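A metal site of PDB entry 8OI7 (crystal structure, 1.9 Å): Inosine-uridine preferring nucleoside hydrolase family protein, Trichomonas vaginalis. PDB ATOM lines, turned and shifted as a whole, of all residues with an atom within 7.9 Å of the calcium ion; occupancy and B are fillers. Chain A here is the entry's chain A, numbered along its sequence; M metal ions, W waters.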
ATOM      1  N   ASP A   8      25.331   7.757 -19.235  1.00  0.00           N
ATOM      2  CA  ASP A   8      26.189   8.136 -18.124  1.00  0.00           C
ATOM      3  C   ASP A   8      26.342   6.925 -17.212  1.00  0.00           C
ATOM      4  O   ASP A   8      25.337   6.416 -16.713  1.00  0.00           O
ATOM      5  CB  ASP A   8      25.605   9.349 -17.396  1.00  0.00           C
ATOM      6  CG  ASP A   8      26.568   9.967 -16.390  1.00  0.00           C
ATOM      7  OD1 ASP A   8      27.515  10.665 -16.821  1.00  0.00           O
ATOM      8  OD2 ASP A   8      26.388   9.702 -15.177  1.00  0.00           O
ATOM      9  N   CYS A   9      27.583   6.477 -16.998  1.00  0.00           N
ATOM     10  CA  CYS A   9      27.801   5.193 -16.342  1.00  0.00           C
ATOM     11  C   CYS A   9      29.176   5.093 -15.699  1.00  0.00           C
ATOM     12  O   CYS A   9      30.021   5.974 -15.852  1.00  0.00           O
ATOM     13  CB  CYS A   9      27.574   4.081 -17.350  1.00  0.00           C
ATOM     14  SG  CYS A   9      28.568   4.287 -18.849  1.00  0.00           S
ATOM     15  N   ASP A  10      29.384   3.976 -14.965  1.00  0.00           N
ATOM     16  CA  ASP A  10      30.613   3.705 -14.229  1.00  0.00           C
ATOM     17  C   ASP A  10      31.060   2.265 -14.486  1.00  0.00           C
ATOM     18  O   ASP A  10      31.176   1.465 -13.553  1.00  0.00           O
ATOM     19  CB  ASP A  10      30.405   3.939 -12.728  1.00  0.00           C
ATOM     20  CG  ASP A  10      29.401   2.995 -12.088  1.00  0.00           C
ATOM     21  OD1 ASP A  10      29.485   2.812 -10.842  1.00  0.00           O
ATOM     22  OD2 ASP A  10      28.541   2.452 -12.830  1.00  0.00           O
ATOM     23  N   PRO A  11      31.347   1.870 -15.747  1.00  0.00           N
ATOM     24  CA  PRO A  11      31.648   0.473 -16.053  1.00  0.00           C
ATOM     25  C   PRO A  11      32.873  -0.030 -15.286  1.00  0.00           C
ATOM     26  O   PRO A  11      33.899   0.666 -15.262  1.00  0.00           O
ATOM     27  CB  PRO A  11      31.908   0.450 -17.576  1.00  0.00           C
ATOM     28  CG  PRO A  11      32.010   1.884 -18.014  1.00  0.00           C
ATOM     29  CD  PRO A  11      31.404   2.744 -16.919  1.00  0.00           C
ATOM     30  N   GLY A  12      32.775  -1.193 -14.629  1.00  0.00           N
ATOM     31  CA  GLY A  12      31.540  -1.883 -14.304  1.00  0.00           C
ATOM     32  C   GLY A  12      31.122  -2.896 -15.366  1.00  0.00           C
ATOM     33  O   GLY A  12      30.896  -2.544 -16.526  1.00  0.00           O
ATOM     34  N   HIS A  13      30.980  -4.158 -14.940  1.00  0.00           N
ATOM     35  CA  HIS A  13      30.559  -5.257 -15.807  1.00  0.00           C
ATOM     36  C   HIS A  13      29.136  -5.025 -16.316  1.00  0.00           C
ATOM     37  O   HIS A  13      28.846  -5.272 -17.487  1.00  0.00           O
ATOM     38  CB  HIS A  13      30.651  -6.595 -15.053  1.00  0.00           C
ATOM     39  CG  HIS A  13      32.021  -6.948 -14.590  1.00  0.00           C
ATOM     40  ND1 HIS A  13      32.713  -6.308 -13.583  1.00  0.00           N
ATOM     41  CD2 HIS A  13      32.820  -7.936 -15.020  1.00  0.00           C
ATOM     42  CE1 HIS A  13      33.904  -6.879 -13.439  1.00  0.00           C
ATOM     43  NE2 HIS A  13      33.989  -7.878 -14.292  1.00  0.00           N
ATOM     44  N   ASP A  14      28.239  -4.594 -15.439  1.00  0.00           N
ATOM     45  CA  ASP A  14      26.854  -4.346 -15.810  1.00  0.00           C
ATOM     46  C   ASP A  14      26.769  -3.216 -16.833  1.00  0.00           C
ATOM     47  O   ASP A  14      26.024  -3.325 -17.815  1.00  0.00           O
ATOM     48  CB  ASP A  14      26.013  -3.978 -14.581  1.00  0.00           C
ATOM     49  CG  ASP A  14      25.888  -5.106 -13.563  1.00  0.00           C
ATOM     50  OD1 ASP A  14      25.094  -6.033 -13.816  1.00  0.00           O
ATOM     51  OD2 ASP A  14      26.592  -5.040 -12.528  1.00  0.00           O
ATOM     52  N   ASP A  15      27.535  -2.137 -16.609  1.00  0.00           N
ATOM     53  CA  ASP A  15      27.498  -0.987 -17.484  1.00  0.00           C
ATOM     54  C   ASP A  15      28.030  -1.387 -18.869  1.00  0.00           C
ATOM     55  O   ASP A  15      27.560  -0.889 -19.886  1.00  0.00           O
ATOM     56  CB  ASP A  15      28.259   0.204 -16.911  1.00  0.00           C
ATOM     57  CG  ASP A  15      27.954   0.540 -15.451  1.00  0.00           C
ATOM     58  OD1 ASP A  15      28.299  -0.285 -14.580  1.00  0.00           O
ATOM     59  OD2 ASP A  15      27.387   1.610 -15.197  1.00  0.00           O
ATOM     60  N   LEU A  16      29.017  -2.279 -18.896  1.00  0.00           N
ATOM     61  CA  LEU A  16      29.554  -2.798 -20.148  1.00  0.00           C
ATOM     62  C   LEU A  16      28.431  -3.412 -20.973  1.00  0.00           C
ATOM     63  O   LEU A  16      28.335  -3.154 -22.168  1.00  0.00           O
ATOM     64  CB  LEU A  16      30.686  -3.795 -19.833  1.00  0.00           C
ATOM     65  CG  LEU A  16      31.163  -4.667 -20.997  1.00  0.00           C
ATOM     66  CD1 LEU A  16      32.658  -4.961 -20.880  1.00  0.00           C
ATOM     67  CD2 LEU A  16      30.391  -5.984 -21.074  1.00  0.00           C
ATOM     68  N   MET A  18      25.253  -2.768 -20.704  1.00  0.00           N
ATOM     69  CA  MET A  18      24.319  -1.698 -21.042  1.00  0.00           C
ATOM     70  C   MET A  18      24.819  -0.937 -22.266  1.00  0.00           C
ATOM     71  O   MET A  18      24.027  -0.599 -23.140  1.00  0.00           O
ATOM     72  CB  MET A  18      24.135  -0.744 -19.846  1.00  0.00           C
ATOM     73  CG  MET A  18      23.136   0.383 -20.099  1.00  0.00           C
ATOM     74  SD  MET A  18      23.864   1.816 -20.919  1.00  0.00           S
ATOM     75  CE  MET A  18      25.085   2.358 -19.734  1.00  0.00           C
ATOM     76  N   THR A  36      31.511   8.326 -14.711  1.00  0.00           N
ATOM     77  CA  THR A  36      31.470   8.896 -13.381  1.00  0.00           C
ATOM     78  C   THR A  36      32.302   8.025 -12.438  1.00  0.00           C
ATOM     79  O   THR A  36      32.689   6.919 -12.793  1.00  0.00           O
ATOM     80  CB  THR A  36      30.012   9.036 -12.900  1.00  0.00           C
ATOM     81  OG1 THR A  36      30.012   9.749 -11.662  1.00  0.00           O
ATOM     82  CG2 THR A  36      29.309   7.708 -12.751  1.00  0.00           C
ATOM     83  N   SER A 141      21.200   6.631 -17.175  1.00  0.00           N
ATOM     84  CA  SER A 141      22.159   6.763 -16.091  1.00  0.00           C
ATOM     85  C   SER A 141      22.216   5.456 -15.297  1.00  0.00           C
ATOM     86  O   SER A 141      21.183   4.984 -14.803  1.00  0.00           O
ATOM     87  CB  SER A 141      21.792   7.931 -15.216  1.00  0.00           C
ATOM     88  OG  SER A 141      22.744   8.100 -14.184  1.00  0.00           O
ATOM     89  N   THR A 142      23.413   4.870 -15.177  1.00  0.00           N
ATOM     90  CA  THR A 142      23.564   3.600 -14.496  1.00  0.00           C
ATOM     91  C   THR A 142      24.735   3.602 -13.513  1.00  0.00           C
ATOM     92  O   THR A 142      25.211   2.546 -13.123  1.00  0.00           O
ATOM     93  CB  THR A 142      23.685   2.449 -15.507  1.00  0.00           C
ATOM     94  OG1 THR A 142      24.890   2.606 -16.251  1.00  0.00           O
ATOM     95  CG2 THR A 142      22.514   2.376 -16.460  1.00  0.00           C
ATOM     96  N   GLY A 143      25.169   4.802 -13.092  1.00  0.00           N
ATOM     97  CA  GLY A 143      26.117   4.952 -12.014  1.00  0.00           C
ATOM     98  C   GLY A 143      25.669   6.035 -11.034  1.00  0.00           C
ATOM     99  O   GLY A 143      24.493   6.370 -11.000  1.00  0.00           O
ATOM    100  N   SER A 144      26.598   6.578 -10.248  1.00  0.00           N
ATOM    101  CA  SER A 144      26.335   7.799  -9.502  1.00  0.00           C
ATOM    102  C   SER A 144      25.785   8.853 -10.474  1.00  0.00           C
ATOM    103  O   SER A 144      26.125   8.833 -11.657  1.00  0.00           O
ATOM    104  CB  SER A 144      27.570   8.327  -8.816  1.00  0.00           C
ATOM    105  OG  SER A 144      28.347   9.098  -9.705  1.00  0.00           O
ATOM    106  N   MET A 167      19.165   3.093 -13.767  1.00  0.00           N
ATOM    107  CA  MET A 167      19.323   1.978 -12.866  1.00  0.00           C
ATOM    108  C   MET A 167      19.805   2.570 -11.543  1.00  0.00           C
ATOM    109  O   MET A 167      20.884   3.173 -11.486  1.00  0.00           O
ATOM    110  CB  MET A 167      20.324   0.960 -13.405  1.00  0.00           C
ATOM    111  CG  MET A 167      20.405  -0.346 -12.605  1.00  0.00           C
ATOM    112  SD  MET A 167      21.298  -0.203 -11.051  1.00  0.00           S
ATOM    113  CE  MET A 167      20.178  -1.037  -9.932  1.00  0.00           C
ATOM    114  N   GLU A 182      20.679   1.475  -2.271  1.00  0.00           N
ATOM    115  CA  GLU A 182      21.357   0.916  -3.424  1.00  0.00           C
ATOM    116  C   GLU A 182      22.551   1.806  -3.771  1.00  0.00           C
ATOM    117  O   GLU A 182      22.498   3.020  -3.608  1.00  0.00           O
ATOM    118  CB  GLU A 182      20.332   0.799  -4.561  1.00  0.00           C
ATOM    119  CG  GLU A 182      20.889   0.293  -5.887  1.00  0.00           C
ATOM    120  CD  GLU A 182      21.607   1.332  -6.726  1.00  0.00           C
ATOM    121  OE1 GLU A 182      21.158   2.500  -6.714  1.00  0.00           O
ATOM    122  OE2 GLU A 182      22.614   0.971  -7.412  1.00  0.00           O
ATOM    123  N   PHE A 183      23.617   1.177  -4.272  1.00  0.00           N
ATOM    124  CA  PHE A 183      24.918   1.786  -4.474  1.00  0.00           C
ATOM    125  C   PHE A 183      24.844   3.138  -5.198  1.00  0.00           C
ATOM    126  O   PHE A 183      25.431   4.119  -4.730  1.00  0.00           O
ATOM    127  CB  PHE A 183      25.807   0.811  -5.245  1.00  0.00           C
ATOM    128  CG  PHE A 183      27.200   1.295  -5.478  1.00  0.00           C
ATOM    129  CD1 PHE A 183      28.122   1.287  -4.442  1.00  0.00           C
ATOM    130  CD2 PHE A 183      27.591   1.798  -6.708  1.00  0.00           C
ATOM    131  CE1 PHE A 183      29.420   1.734  -4.640  1.00  0.00           C
ATOM    132  CE2 PHE A 183      28.882   2.250  -6.912  1.00  0.00           C
ATOM    133  CZ  PHE A 183      29.792   2.224  -5.875  1.00  0.00           C
ATOM    134  N   ASN A 184      24.173   3.164  -6.364  1.00  0.00           N
ATOM    135  CA  ASN A 184      24.156   4.343  -7.219  1.00  0.00           C
ATOM    136  C   ASN A 184      23.567   5.560  -6.521  1.00  0.00           C
ATOM    137  O   ASN A 184      23.950   6.683  -6.844  1.00  0.00           O
ATOM    138  CB  ASN A 184      23.421   4.080  -8.540  1.00  0.00           C
ATOM    139  CG  ASN A 184      24.196   3.137  -9.439  1.00  0.00           C
ATOM    140  OD1 ASN A 184      25.387   2.918  -9.225  1.00  0.00           O
ATOM    141  ND2 ASN A 184      23.533   2.586 -10.437  1.00  0.00           N
ATOM    142  N   HIS A 262      22.083  -5.914 -14.050  1.00  0.00           N
ATOM    143  CA  HIS A 262      21.377  -4.717 -13.622  1.00  0.00           C
ATOM    144  C   HIS A 262      21.232  -3.726 -14.777  1.00  0.00           C
ATOM    145  O   HIS A 262      20.167  -3.629 -15.398  1.00  0.00           O
ATOM    146  CB  HIS A 262      22.116  -4.055 -12.443  1.00  0.00           C
ATOM    147  CG  HIS A 262      22.271  -4.883 -11.220  1.00  0.00           C
ATOM    148  ND1 HIS A 262      21.315  -4.988 -10.238  1.00  0.00           N
ATOM    149  CD2 HIS A 262      23.319  -5.590 -10.781  1.00  0.00           C
ATOM    150  CE1 HIS A 262      21.762  -5.761  -9.261  1.00  0.00           C
ATOM    151  NE2 HIS A 262      22.968  -6.144  -9.577  1.00  0.00           N
ATOM    152  N   ASP A 263      22.321  -3.014 -15.076  1.00  0.00           N
ATOM    153  CA  ASP A 263      22.301  -1.767 -15.821  1.00  0.00           C
ATOM    154  C   ASP A 263      21.643  -1.860 -17.199  1.00  0.00           C
ATOM    155  O   ASP A 263      20.949  -0.929 -17.589  1.00  0.00           O
ATOM    156  CB  ASP A 263      23.723  -1.206 -15.941  1.00  0.00           C
ATOM    157  CG  ASP A 263      24.342  -0.876 -14.591  1.00  0.00           C
ATOM    158  OD1 ASP A 263      23.714  -1.161 -13.568  1.00  0.00           O
ATOM    159  OD2 ASP A 263      25.451  -0.349 -14.571  1.00  0.00           O
HETATM  160 CA    CA M   1      26.813   0.779 -12.948  1.00  0.00          CA
HETATM  161  O   HOH W   1      24.995   0.053 -11.519  1.00  0.00           O
HETATM  162  O   HOH W   2      27.760  -1.220 -11.974  1.00  0.00           O
HETATM  163  O   HOH W   3      27.079   1.496 -10.627  1.00  0.00           O
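Water W3 bridges OD1 of Asn 184 and OD1 of Asp 10.
Water W1 lies within hydrogen-bond range of OD1 of Asp 263 (2.7 Å), ND2 of Asn 184 (3.1 Å) and SD of Met 167 (3.7 Å).
Four residues have an atom within 4 Å of the calcium ion: Asp 10, Asp 15, Thr 142 and Asp 263.
The nearest printed residue that does not touch the calcium ion is Gly 143 (4.3 Å).
The backbone carbonyl oxygen of Thr 142 lies close to the side-chain amide nitrogen of Asn 184, 3.2 Å away.
The backbone carbonyl oxygen of Asp 8 lies within hydrogen-bond range of the backbone NH of Thr 142 (2.9 Å).
The calcium ion is bound by the backbone carbonyl oxygen (O) of Thr 142 (2.4 Å), the side-chain carboxylate (OD2) of Asp 263 (2.4 Å), the side-chain carboxylate (OD2) of Asp 10 (2.4 Å), water W2 (2.4 Å), water W1 (2.4 Å), water W3 (2.4 Å), the side-chain carboxylate (OD1) of Asp 15 (2.5 Å) and the side-chain carboxylate (OD2) of Asp 15 (2.5 Å).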
